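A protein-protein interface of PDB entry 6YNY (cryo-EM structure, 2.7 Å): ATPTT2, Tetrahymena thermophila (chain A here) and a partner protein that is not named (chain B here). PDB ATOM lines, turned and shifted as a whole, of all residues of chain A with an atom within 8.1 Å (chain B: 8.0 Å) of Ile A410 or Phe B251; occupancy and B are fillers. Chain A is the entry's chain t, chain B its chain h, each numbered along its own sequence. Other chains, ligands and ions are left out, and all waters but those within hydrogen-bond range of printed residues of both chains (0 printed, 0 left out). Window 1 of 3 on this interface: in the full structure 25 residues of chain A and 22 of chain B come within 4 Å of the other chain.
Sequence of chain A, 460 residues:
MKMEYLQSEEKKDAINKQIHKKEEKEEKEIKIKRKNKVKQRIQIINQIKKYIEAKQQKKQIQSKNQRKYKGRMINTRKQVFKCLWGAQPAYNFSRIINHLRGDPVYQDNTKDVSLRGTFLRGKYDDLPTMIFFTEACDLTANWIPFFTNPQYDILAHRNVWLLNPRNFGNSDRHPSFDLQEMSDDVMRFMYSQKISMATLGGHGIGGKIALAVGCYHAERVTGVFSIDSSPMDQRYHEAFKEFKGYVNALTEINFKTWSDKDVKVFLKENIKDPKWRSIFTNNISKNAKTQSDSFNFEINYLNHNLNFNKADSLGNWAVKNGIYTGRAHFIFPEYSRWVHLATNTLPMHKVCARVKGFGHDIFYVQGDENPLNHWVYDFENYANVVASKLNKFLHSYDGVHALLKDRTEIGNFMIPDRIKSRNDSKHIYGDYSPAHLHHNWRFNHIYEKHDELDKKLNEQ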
ATOM      1  N   HIS A 395       2.706  18.754   2.499  1.00  0.00           N
ATOM      2  CA  HIS A 395       3.034  19.995   1.814  1.00  0.00           C
ATOM      3  C   HIS A 395       3.873  20.925   2.683  1.00  0.00           C
ATOM      4  O   HIS A 395       4.820  21.546   2.190  1.00  0.00           O
ATOM      5  CB  HIS A 395       1.754  20.700   1.373  1.00  0.00           C
ATOM      6  CG  HIS A 395       1.995  21.938   0.572  1.00  0.00           C
ATOM      7  ND1 HIS A 395       2.441  21.906  -0.730  1.00  0.00           N
ATOM      8  CD2 HIS A 395       1.855  23.246   0.889  1.00  0.00           C
ATOM      9  CE1 HIS A 395       2.562  23.140  -1.183  1.00  0.00           C
ATOM     10  NE2 HIS A 395       2.214  23.972  -0.220  1.00  0.00           N
ATOM     11  N   SER A 396       3.540  21.046   3.965  1.00  0.00           N
ATOM     12  CA  SER A 396       4.128  22.066   4.817  1.00  0.00           C
ATOM     13  C   SER A 396       4.981  21.537   5.961  1.00  0.00           C
ATOM     14  O   SER A 396       5.894  22.242   6.393  1.00  0.00           O
ATOM     15  CB  SER A 396       3.024  22.954   5.403  1.00  0.00           C
ATOM     16  OG  SER A 396       2.029  22.178   6.037  1.00  0.00           O
ATOM     17  N   ASP A 398       6.077  17.815   6.505  1.00  0.00           N
ATOM     18  CA  ASP A 398       6.928  16.648   6.336  1.00  0.00           C
ATOM     19  C   ASP A 398       8.263  17.044   5.722  1.00  0.00           C
ATOM     20  O   ASP A 398       8.327  17.847   4.788  1.00  0.00           O
ATOM     21  CB  ASP A 398       6.239  15.606   5.463  1.00  0.00           C
ATOM     22  CG  ASP A 398       7.069  14.360   5.284  1.00  0.00           C
ATOM     23  OD1 ASP A 398       8.048  14.181   6.034  1.00  0.00           O
ATOM     24  OD2 ASP A 398       6.751  13.567   4.377  1.00  0.00           O
ATOM     25  N   GLY A 399       9.333  16.463   6.256  1.00  0.00           N
ATOM     26  CA  GLY A 399      10.668  16.745   5.775  1.00  0.00           C
ATOM     27  C   GLY A 399      11.117  18.160   6.040  1.00  0.00           C
ATOM     28  O   GLY A 399      11.901  18.712   5.266  1.00  0.00           O
ATOM     29  N   VAL A 400      10.643  18.757   7.126  1.00  0.00           N
ATOM     30  CA  VAL A 400      11.032  20.096   7.539  1.00  0.00           C
ATOM     31  C   VAL A 400      11.809  19.985   8.839  1.00  0.00           C
ATOM     32  O   VAL A 400      11.460  19.190   9.719  1.00  0.00           O
ATOM     33  CB  VAL A 400       9.809  21.016   7.705  1.00  0.00           C
ATOM     34  CG1 VAL A 400      10.233  22.364   8.216  1.00  0.00           C
ATOM     35  CG2 VAL A 400       9.092  21.171   6.396  1.00  0.00           C
ATOM     36  N   HIS A 401      12.870  20.774   8.952  1.00  0.00           N
ATOM     37  CA  HIS A 401      13.706  20.740  10.141  1.00  0.00           C
ATOM     38  C   HIS A 401      12.864  20.997  11.384  1.00  0.00           C
ATOM     39  O   HIS A 401      11.865  21.719  11.350  1.00  0.00           O
ATOM     40  CB  HIS A 401      14.821  21.775  10.028  1.00  0.00           C
ATOM     41  CG  HIS A 401      15.905  21.609  11.045  1.00  0.00           C
ATOM     42  ND1 HIS A 401      15.822  22.132  12.315  1.00  0.00           N
ATOM     43  CD2 HIS A 401      17.103  20.985  10.972  1.00  0.00           C
ATOM     44  CE1 HIS A 401      16.920  21.832  12.985  1.00  0.00           C
ATOM     45  NE2 HIS A 401      17.714  21.136  12.192  1.00  0.00           N
ATOM     46  N   LEU A 404      12.183  24.593  12.679  1.00  0.00           N
ATOM     47  CA  LEU A 404      11.405  25.408  11.762  1.00  0.00           C
ATOM     48  C   LEU A 404       9.928  25.082  11.926  1.00  0.00           C
ATOM     49  O   LEU A 404       9.554  23.923  12.120  1.00  0.00           O
ATOM     50  CB  LEU A 404      11.836  25.175  10.314  1.00  0.00           C
ATOM     51  CG  LEU A 404      13.313  25.390   9.991  1.00  0.00           C
ATOM     52  CD1 LEU A 404      13.521  25.378   8.496  1.00  0.00           C
ATOM     53  CD2 LEU A 404      13.836  26.663  10.585  1.00  0.00           C
ATOM     54  N   LYS A 405       9.091  26.114  11.854  1.00  0.00           N
ATOM     55  CA  LYS A 405       7.653  25.905  11.966  1.00  0.00           C
ATOM     56  C   LYS A 405       7.121  25.129  10.771  1.00  0.00           C
ATOM     57  O   LYS A 405       6.543  24.048  10.918  1.00  0.00           O
ATOM     58  CB  LYS A 405       6.934  27.248  12.079  1.00  0.00           C
ATOM     59  CG  LYS A 405       7.012  27.899  13.436  1.00  0.00           C
ATOM     60  CD  LYS A 405       6.313  27.100  14.519  1.00  0.00           C
ATOM     61  CE  LYS A 405       4.858  26.889  14.217  1.00  0.00           C
ATOM     62  NZ  LYS A 405       4.170  26.261  15.365  1.00  0.00           N
ATOM     63  N   ASP A 406       7.312  25.674   9.574  1.00  0.00           N
ATOM     64  CA  ASP A 406       6.715  25.138   8.365  1.00  0.00           C
ATOM     65  C   ASP A 406       7.744  25.182   7.249  1.00  0.00           C
ATOM     66  O   ASP A 406       8.885  25.611   7.439  1.00  0.00           O
ATOM     67  CB  ASP A 406       5.469  25.933   7.968  1.00  0.00           C
ATOM     68  CG  ASP A 406       4.528  26.148   9.120  1.00  0.00           C
ATOM     69  OD1 ASP A 406       4.257  25.177   9.855  1.00  0.00           O
ATOM     70  OD2 ASP A 406       4.072  27.297   9.301  1.00  0.00           O
ATOM     71  N   ARG A 407       7.325  24.731   6.070  1.00  0.00           N
ATOM     72  CA  ARG A 407       8.174  24.821   4.894  1.00  0.00           C
ATOM     73  C   ARG A 407       8.358  26.264   4.452  1.00  0.00           C
ATOM     74  O   ARG A 407       9.330  26.573   3.757  1.00  0.00           O
ATOM     75  CB  ARG A 407       7.575  23.987   3.769  1.00  0.00           C
ATOM     76  CG  ARG A 407       8.589  23.449   2.808  1.00  0.00           C
ATOM     77  CD  ARG A 407       7.991  22.404   1.899  1.00  0.00           C
ATOM     78  NE  ARG A 407       9.025  21.615   1.247  1.00  0.00           N
ATOM     79  CZ  ARG A 407       9.590  20.543   1.787  1.00  0.00           C
ATOM     80  NH1 ARG A 407       9.230  20.124   2.985  1.00  0.00           N
ATOM     81  NH2 ARG A 407      10.520  19.888   1.123  1.00  0.00           N
ATOM     82  N   THR A 408       7.437  27.146   4.842  1.00  0.00           N
ATOM     83  CA  THR A 408       7.553  28.561   4.512  1.00  0.00           C
ATOM     84  C   THR A 408       8.820  29.176   5.089  1.00  0.00           C
ATOM     85  O   THR A 408       9.362  30.127   4.517  1.00  0.00           O
ATOM     86  CB  THR A 408       6.330  29.312   5.032  1.00  0.00           C
ATOM     87  OG1 THR A 408       6.122  28.984   6.411  1.00  0.00           O
ATOM     88  CG2 THR A 408       5.097  28.948   4.238  1.00  0.00           C
ATOM     89  N   GLU A 409       9.299  28.661   6.219  1.00  0.00           N
ATOM     90  CA  GLU A 409      10.467  29.221   6.884  1.00  0.00           C
ATOM     91  C   GLU A 409      11.782  28.772   6.267  1.00  0.00           C
ATOM     92  O   GLU A 409      12.840  29.233   6.707  1.00  0.00           O
ATOM     93  CB  GLU A 409      10.455  28.857   8.371  1.00  0.00           C
ATOM     94  CG  GLU A 409       9.485  29.672   9.195  1.00  0.00           C
ATOM     95  CD  GLU A 409       9.733  29.548  10.680  1.00  0.00           C
ATOM     96  OE1 GLU A 409      10.418  28.589  11.094  1.00  0.00           O
ATOM     97  OE2 GLU A 409       9.252  30.415  11.437  1.00  0.00           O
ATOM     98  N   ILE A 410      11.752  27.889   5.272  1.00  0.00           N
ATOM     99  CA  ILE A 410      12.983  27.443   4.633  1.00  0.00           C
ATOM    100  C   ILE A 410      13.589  28.607   3.862  1.00  0.00           C
ATOM    101  O   ILE A 410      12.977  29.143   2.931  1.00  0.00           O
ATOM    102  CB  ILE A 410      12.723  26.243   3.716  1.00  0.00           C
ATOM    103  CG1 ILE A 410      12.350  25.023   4.551  1.00  0.00           C
ATOM    104  CG2 ILE A 410      13.946  25.950   2.877  1.00  0.00           C
ATOM    105  CD1 ILE A 410      12.015  23.802   3.744  1.00  0.00           C
ATOM    106  N   GLY A 411      14.804  28.997   4.244  1.00  0.00           N
ATOM    107  CA  GLY A 411      15.511  30.076   3.599  1.00  0.00           C
ATOM    108  C   GLY A 411      15.320  31.440   4.219  1.00  0.00           C
ATOM    109  O   GLY A 411      15.988  32.391   3.796  1.00  0.00           O
ATOM    110  N   ASN A 412      14.435  31.575   5.205  1.00  0.00           N
ATOM    111  CA  ASN A 412      14.216  32.854   5.862  1.00  0.00           C
ATOM    112  C   ASN A 412      14.282  32.790   7.380  1.00  0.00           C
ATOM    113  O   ASN A 412      14.297  33.850   8.015  1.00  0.00           O
ATOM    114  CB  ASN A 412      12.862  33.448   5.452  1.00  0.00           C
ATOM    115  CG  ASN A 412      11.702  32.553   5.804  1.00  0.00           C
ATOM    116  OD1 ASN A 412      11.137  32.643   6.892  1.00  0.00           O
ATOM    117  ND2 ASN A 412      11.330  31.684   4.877  1.00  0.00           N
ATOM    118  N   PHE A 413      14.323  31.605   7.979  1.00  0.00           N
ATOM    119  CA  PHE A 413      14.467  31.460   9.418  1.00  0.00           C
ATOM    120  C   PHE A 413      15.813  30.823   9.719  1.00  0.00           C
ATOM    121  O   PHE A 413      16.154  29.782   9.149  1.00  0.00           O
ATOM    122  CB  PHE A 413      13.340  30.620  10.015  1.00  0.00           C
ATOM    123  CG  PHE A 413      13.371  30.555  11.510  1.00  0.00           C
ATOM    124  CD1 PHE A 413      12.806  31.557  12.266  1.00  0.00           C
ATOM    125  CD2 PHE A 413      13.972  29.497  12.159  1.00  0.00           C
ATOM    126  CE1 PHE A 413      12.837  31.504  13.637  1.00  0.00           C
ATOM    127  CE2 PHE A 413      14.005  29.440  13.532  1.00  0.00           C
ATOM    128  CZ  PHE A 413      13.437  30.444  14.270  1.00  0.00           C
ATOM    129  N   MET A 414      16.569  31.449  10.612  1.00  0.00           N
ATOM    130  CA  MET A 414      17.908  31.007  10.960  1.00  0.00           C
ATOM    131  C   MET A 414      17.893  30.383  12.345  1.00  0.00           C
ATOM    132  O   MET A 414      17.347  30.963  13.289  1.00  0.00           O
ATOM    133  CB  MET A 414      18.892  32.174  10.908  1.00  0.00           C
ATOM    134  CG  MET A 414      19.127  32.713   9.519  1.00  0.00           C
ATOM    135  SD  MET A 414      20.154  31.642   8.515  1.00  0.00           S
ATOM    136  CE  MET A 414      20.192  32.584   7.004  1.00  0.00           C
ATOM    137  N   SER A 433      20.560  28.718   8.491  1.00  0.00           N
ATOM    138  CA  SER A 433      19.408  27.988   7.996  1.00  0.00           C
ATOM    139  C   SER A 433      19.818  26.552   7.702  1.00  0.00           C
ATOM    140  O   SER A 433      20.733  26.336   6.898  1.00  0.00           O
ATOM    141  CB  SER A 433      18.861  28.640   6.742  1.00  0.00           C
ATOM    142  OG  SER A 433      19.792  28.569   5.684  1.00  0.00           O
ATOM    143  N   PRO A 434      19.192  25.553   8.316  1.00  0.00           N
ATOM    144  CA  PRO A 434      19.669  24.182   8.144  1.00  0.00           C
ATOM    145  C   PRO A 434      19.486  23.699   6.716  1.00  0.00           C
ATOM    146  O   PRO A 434      18.627  24.179   5.975  1.00  0.00           O
ATOM    147  CB  PRO A 434      18.805  23.382   9.122  1.00  0.00           C
ATOM    148  CG  PRO A 434      17.584  24.175   9.263  1.00  0.00           C
ATOM    149  CD  PRO A 434      17.995  25.605   9.169  1.00  0.00           C
ATOM    150  N   ALA A 435      20.317  22.736   6.336  1.00  0.00           N
ATOM    151  CA  ALA A 435      20.299  22.215   4.981  1.00  0.00           C
ATOM    152  C   ALA A 435      19.175  21.207   4.806  1.00  0.00           C
ATOM    153  O   ALA A 435      19.043  20.261   5.588  1.00  0.00           O
ATOM    154  CB  ALA A 435      21.636  21.562   4.645  1.00  0.00           C
ATOM    155  N   HIS A 436      18.363  21.419   3.778  1.00  0.00           N
ATOM    156  CA  HIS A 436      17.343  20.474   3.354  1.00  0.00           C
ATOM    157  C   HIS A 436      17.758  19.931   1.996  1.00  0.00           C
ATOM    158  O   HIS A 436      17.948  20.701   1.050  1.00  0.00           O
ATOM    159  CB  HIS A 436      15.969  21.135   3.285  1.00  0.00           C
ATOM    160  CG  HIS A 436      15.449  21.601   4.606  1.00  0.00           C
ATOM    161  ND1 HIS A 436      16.066  22.585   5.345  1.00  0.00           N
ATOM    162  CD2 HIS A 436      14.365  21.218   5.319  1.00  0.00           C
ATOM    163  CE1 HIS A 436      15.384  22.788   6.458  1.00  0.00           C
ATOM    164  NE2 HIS A 436      14.348  21.971   6.467  1.00  0.00           N
ATOM    165  N   LEU A 437      17.907  18.616   1.903  1.00  0.00           N
ATOM    166  CA  LEU A 437      18.468  17.980   0.724  1.00  0.00           C
ATOM    167  C   LEU A 437      17.371  17.433  -0.182  1.00  0.00           C
ATOM    168  O   LEU A 437      16.199  17.353   0.186  1.00  0.00           O
ATOM    169  CB  LEU A 437      19.422  16.859   1.135  1.00  0.00           C
ATOM    170  CG  LEU A 437      20.528  17.244   2.111  1.00  0.00           C
ATOM    171  CD1 LEU A 437      21.320  16.024   2.492  1.00  0.00           C
ATOM    172  CD2 LEU A 437      21.435  18.293   1.521  1.00  0.00           C
ATOM    173  N   HIS A 438      17.778  17.049  -1.388  1.00  0.00           N
ATOM    174  CA  HIS A 438      16.861  16.438  -2.335  1.00  0.00           C
ATOM    175  C   HIS A 438      16.447  15.055  -1.846  1.00  0.00           C
ATOM    176  O   HIS A 438      17.194  14.371  -1.141  1.00  0.00           O
ATOM    177  CB  HIS A 438      17.513  16.346  -3.711  1.00  0.00           C
ATOM    178  CG  HIS A 438      16.539  16.177  -4.833  1.00  0.00           C
ATOM    179  ND1 HIS A 438      16.063  14.946  -5.228  1.00  0.00           N
ATOM    180  CD2 HIS A 438      15.958  17.086  -5.649  1.00  0.00           C
ATOM    181  CE1 HIS A 438      15.225  15.106  -6.237  1.00  0.00           C
ATOM    182  NE2 HIS A 438      15.144  16.394  -6.512  1.00  0.00           N
ATOM    183  N   TYR A 447      23.086  17.208  -7.613  1.00  0.00           N
ATOM    184  CA  TYR A 447      24.047  18.141  -7.036  1.00  0.00           C
ATOM    185  C   TYR A 447      25.247  18.324  -7.952  1.00  0.00           C
ATOM    186  O   TYR A 447      25.721  19.448  -8.146  1.00  0.00           O
ATOM    187  CB  TYR A 447      24.482  17.658  -5.654  1.00  0.00           C
ATOM    188  CG  TYR A 447      23.464  17.962  -4.588  1.00  0.00           C
ATOM    189  CD1 TYR A 447      23.345  19.237  -4.068  1.00  0.00           C
ATOM    190  CD2 TYR A 447      22.615  16.980  -4.108  1.00  0.00           C
ATOM    191  CE1 TYR A 447      22.418  19.527  -3.105  1.00  0.00           C
ATOM    192  CE2 TYR A 447      21.682  17.263  -3.140  1.00  0.00           C
ATOM    193  CZ  TYR A 447      21.588  18.538  -2.644  1.00  0.00           C
ATOM    194  OH  TYR A 447      20.661  18.834  -1.678  1.00  0.00           O
ATOM    195  N   ALA B 232       6.950  30.765  -6.345  1.00  0.00           N
ATOM    196  CA  ALA B 232       8.250  30.454  -5.771  1.00  0.00           C
ATOM    197  C   ALA B 232       9.383  31.110  -6.543  1.00  0.00           C
ATOM    198  O   ALA B 232      10.486  31.250  -6.005  1.00  0.00           O
ATOM    199  CB  ALA B 232       8.452  28.944  -5.734  1.00  0.00           C
ATOM    200  N   VAL B 235      10.756  34.802  -5.043  1.00  0.00           N
ATOM    201  CA  VAL B 235      11.780  34.799  -4.006  1.00  0.00           C
ATOM    202  C   VAL B 235      13.078  34.203  -4.532  1.00  0.00           C
ATOM    203  O   VAL B 235      14.169  34.628  -4.133  1.00  0.00           O
ATOM    204  CB  VAL B 235      11.276  34.054  -2.757  1.00  0.00           C
ATOM    205  CG1 VAL B 235      10.106  34.796  -2.141  1.00  0.00           C
ATOM    206  CG2 VAL B 235      10.879  32.634  -3.095  1.00  0.00           C
ATOM    207  N   ARG B 236      12.990  33.221  -5.425  1.00  0.00           N
ATOM    208  CA  ARG B 236      14.158  32.598  -6.043  1.00  0.00           C
ATOM    209  C   ARG B 236      13.996  32.669  -7.554  1.00  0.00           C
ATOM    210  O   ARG B 236      13.421  31.762  -8.171  1.00  0.00           O
ATOM    211  CB  ARG B 236      14.321  31.159  -5.569  1.00  0.00           C
ATOM    212  CG  ARG B 236      14.488  31.045  -4.076  1.00  0.00           C
ATOM    213  CD  ARG B 236      14.478  29.615  -3.605  1.00  0.00           C
ATOM    214  NE  ARG B 236      13.946  29.511  -2.252  1.00  0.00           N
ATOM    215  CZ  ARG B 236      12.658  29.357  -1.967  1.00  0.00           C
ATOM    216  NH1 ARG B 236      11.756  29.279  -2.935  1.00  0.00           N
ATOM    217  NH2 ARG B 236      12.268  29.279  -0.705  1.00  0.00           N
ATOM    218  N   ASP B 245      13.157  28.811  -9.217  1.00  0.00           N
ATOM    219  CA  ASP B 245      13.353  27.966  -8.043  1.00  0.00           C
ATOM    220  C   ASP B 245      13.711  26.541  -8.455  1.00  0.00           C
ATOM    221  O   ASP B 245      13.092  25.566  -8.024  1.00  0.00           O
ATOM    222  CB  ASP B 245      12.112  27.986  -7.156  1.00  0.00           C
ATOM    223  CG  ASP B 245      12.348  27.338  -5.811  1.00  0.00           C
ATOM    224  OD1 ASP B 245      13.467  26.844  -5.569  1.00  0.00           O
ATOM    225  OD2 ASP B 245      11.412  27.331  -4.991  1.00  0.00           O
ATOM    226  N   GLY B 246      14.723  26.424  -9.309  1.00  0.00           N
ATOM    227  CA  GLY B 246      15.158  25.128  -9.785  1.00  0.00           C
ATOM    228  C   GLY B 246      16.551  24.725  -9.355  1.00  0.00           C
ATOM    229  O   GLY B 246      17.126  23.797  -9.930  1.00  0.00           O
ATOM    230  N   ASN B 247      17.111  25.403  -8.357  1.00  0.00           N
ATOM    231  CA  ASN B 247      18.455  25.121  -7.873  1.00  0.00           C
ATOM    232  C   ASN B 247      18.385  24.482  -6.494  1.00  0.00           C
ATOM    233  O   ASN B 247      17.768  25.037  -5.579  1.00  0.00           O
ATOM    234  CB  ASN B 247      19.290  26.398  -7.815  1.00  0.00           C
ATOM    235  CG  ASN B 247      20.753  26.124  -7.573  1.00  0.00           C
ATOM    236  OD1 ASN B 247      21.124  25.089  -7.025  1.00  0.00           O
ATOM    237  ND2 ASN B 247      21.598  27.057  -7.981  1.00  0.00           N
ATOM    238  N   VAL B 248      19.023  23.318  -6.350  1.00  0.00           N
ATOM    239  CA  VAL B 248      19.074  22.655  -5.052  1.00  0.00           C
ATOM    240  C   VAL B 248      20.050  23.353  -4.119  1.00  0.00           C
ATOM    241  O   VAL B 248      19.874  23.332  -2.896  1.00  0.00           O
ATOM    242  CB  VAL B 248      19.445  21.170  -5.218  1.00  0.00           C
ATOM    243  CG1 VAL B 248      18.357  20.431  -5.937  1.00  0.00           C
ATOM    244  CG2 VAL B 248      20.757  21.023  -5.962  1.00  0.00           C
ATOM    245  N   ASN B 249      21.093  23.975  -4.668  1.00  0.00           N
ATOM    246  CA  ASN B 249      22.117  24.586  -3.834  1.00  0.00           C
ATOM    247  C   ASN B 249      21.569  25.730  -2.997  1.00  0.00           C
ATOM    248  O   ASN B 249      22.142  26.048  -1.950  1.00  0.00           O
ATOM    249  CB  ASN B 249      23.271  25.066  -4.707  1.00  0.00           C
ATOM    250  CG  ASN B 249      23.920  23.941  -5.481  1.00  0.00           C
ATOM    251  OD1 ASN B 249      23.999  22.809  -5.007  1.00  0.00           O
ATOM    252  ND2 ASN B 249      24.389  24.245  -6.681  1.00  0.00           N
ATOM    253  N   ASP B 250      20.477  26.357  -3.433  1.00  0.00           N
ATOM    254  CA  ASP B 250      19.884  27.438  -2.657  1.00  0.00           C
ATOM    255  C   ASP B 250      19.389  26.948  -1.304  1.00  0.00           C
ATOM    256  O   ASP B 250      19.302  27.733  -0.354  1.00  0.00           O
ATOM    257  CB  ASP B 250      18.736  28.075  -3.435  1.00  0.00           C
ATOM    258  CG  ASP B 250      19.196  28.734  -4.714  1.00  0.00           C
ATOM    259  OD1 ASP B 250      20.384  29.110  -4.796  1.00  0.00           O
ATOM    260  OD2 ASP B 250      18.369  28.880  -5.637  1.00  0.00           O
ATOM    261  N   PHE B 251      19.055  25.665  -1.198  1.00  0.00           N
ATOM    262  CA  PHE B 251      18.507  25.098   0.022  1.00  0.00           C
ATOM    263  C   PHE B 251      19.557  24.411   0.883  1.00  0.00           C
ATOM    264  O   PHE B 251      19.202  23.741   1.856  1.00  0.00           O
ATOM    265  CB  PHE B 251      17.388  24.124  -0.326  1.00  0.00           C
ATOM    266  CG  PHE B 251      16.329  24.727  -1.185  1.00  0.00           C
ATOM    267  CD1 PHE B 251      15.321  25.487  -0.632  1.00  0.00           C
ATOM    268  CD2 PHE B 251      16.355  24.556  -2.553  1.00  0.00           C
ATOM    269  CE1 PHE B 251      14.356  26.052  -1.424  1.00  0.00           C
ATOM    270  CE2 PHE B 251      15.391  25.118  -3.349  1.00  0.00           C
ATOM    271  CZ  PHE B 251      14.391  25.869  -2.785  1.00  0.00           C
ATOM    272  N   LEU B 252      20.835  24.554   0.548  1.00  0.00           N
ATOM    273  CA  LEU B 252      21.888  24.101   1.438  1.00  0.00           C
ATOM    274  C   LEU B 252      22.043  25.091   2.589  1.00  0.00           C
ATOM    275  O   LEU B 252      21.387  26.134   2.639  1.00  0.00           O
ATOM    276  CB  LEU B 252      23.197  23.930   0.673  1.00  0.00           C
ATOM    277  CG  LEU B 252      23.217  22.853  -0.409  1.00  0.00           C
ATOM    278  CD1 LEU B 252      24.508  22.909  -1.185  1.00  0.00           C
ATOM    279  CD2 LEU B 252      23.033  21.483   0.197  1.00  0.00           C
ATOM    280  N   GLU B 253      22.916  24.759   3.534  1.00  0.00           N
ATOM    281  CA  GLU B 253      23.081  25.592   4.716  1.00  0.00           C
ATOM    282  C   GLU B 253      23.528  26.992   4.326  1.00  0.00           C
ATOM    283  O   GLU B 253      24.533  27.169   3.631  1.00  0.00           O
ATOM    284  CB  GLU B 253      24.081  24.957   5.679  1.00  0.00           C
ATOM    285  CG  GLU B 253      24.365  25.791   6.909  1.00  0.00           C
ATOM    286  CD  GLU B 253      25.104  25.030   7.986  1.00  0.00           C
ATOM    287  OE1 GLU B 253      24.811  23.832   8.179  1.00  0.00           O
ATOM    288  OE2 GLU B 253      25.977  25.630   8.644  1.00  0.00           O
ATOM    289  N   GLN B 254      22.775  27.989   4.777  1.00  0.00           N
ATOM    290  CA  GLN B 254      23.067  29.385   4.505  1.00  0.00           C
ATOM    291  C   GLN B 254      23.301  30.119   5.815  1.00  0.00           C
ATOM    292  O   GLN B 254      22.949  29.639   6.896  1.00  0.00           O
ATOM    293  CB  GLN B 254      21.929  30.061   3.732  1.00  0.00           C
ATOM    294  CG  GLN B 254      21.701  29.503   2.350  1.00  0.00           C
ATOM    295  CD  GLN B 254      22.889  29.702   1.439  1.00  0.00           C
ATOM    296  OE1 GLN B 254      23.763  30.524   1.708  1.00  0.00           O
ATOM    297  NE2 GLN B 254      22.929  28.944   0.352  1.00  0.00           N
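Of the 24 printed residues of chain A, 7 touch a printed residue of chain B. Printed residues of chain A that touch a printed residue of chain B: Ile A410, Met A414, Ser A433, Ala A435, His A436, Leu A437 and Tyr A447. Printed residues of chain B that touch a printed residue of chain A: Arg B236, Val B248, Asn B249, Phe B251, Leu B252, Glu B253 and Gln B254. Among the printed residues, 12 pairs touch across the chains. Among the printed residues, no Asp or Glu carboxylate lies within 4 Å of a Lys or Arg side-chain nitrogen of the other chain.
Ile A410 touches just these residues of chain B: Arg B236 (3.7 Å) and Phe B251 (3.8 Å). Printed residues of chain B within 4 Å of Ser A433: Glu B253 and Gln B254. Of the printed residues of chain B, His A436 touches Phe B251 (3.1 Å). Gly B246 touches none of the printed residues of chain A. Phe B251 touches just these residues of chain A: Ile A410, Ala A435 and His A436. Printed residues of chain A within 4 Å of Leu B252: Leu A437 and Tyr A447. The nearest residue of chain B that does not touch Ile A410 is Asp B250 (6.5 Å). The nearest printed residue of chain A that does not touch Val B248 is His A438 (4.1 Å).
N of His A401 is in hydrogen-bond range of NE2 of His A436 (3.1 Å). SD of Met A414 is in hydrogen-bond range of N of Ser A433 (3.0 Å). ND1 of His A436 is in hydrogen-bond range of O of Pro A434. N of His A438 sits at hydrogen-bond distance from OH of Tyr A447 (3.4 Å). The side-chain carboxylate (OD2) of Asp B245 is in salt-bridge range of the guanidinium group (NH1) of Arg B236 (2.9 Å). The side-chain amide oxygen (OD1) of Asn B247 lies within hydrogen-bond range of the backbone NH (N) of Asn B249 (2.6 Å).
O of Gln B254 is in hydrogen-bond range of N of Ser A433, 3.0 Å away. N of His A436 sits at hydrogen-bond distance from O of Phe B251 (3.1 Å).
Among the printed residues, pairs that only touch across the chains: Ile A410 with Arg B236 (3.7 Å), Ile A410 with Phe B251 (3.8 Å), Met A414 with Gln B254 (3.8 Å), Ser A433 with Glu B253 (3.3 Å), Ala A435 with Phe B251 (3.6 Å), Ala A435 with Glu B253 (3.6 Å), Leu A437 with Leu B252 (3.8 Å), Tyr A447 with Val B248 (3.6 Å), Tyr A447 with Asn B249 (3.8 Å) and Tyr A447 with Leu B252 (3.9 Å).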
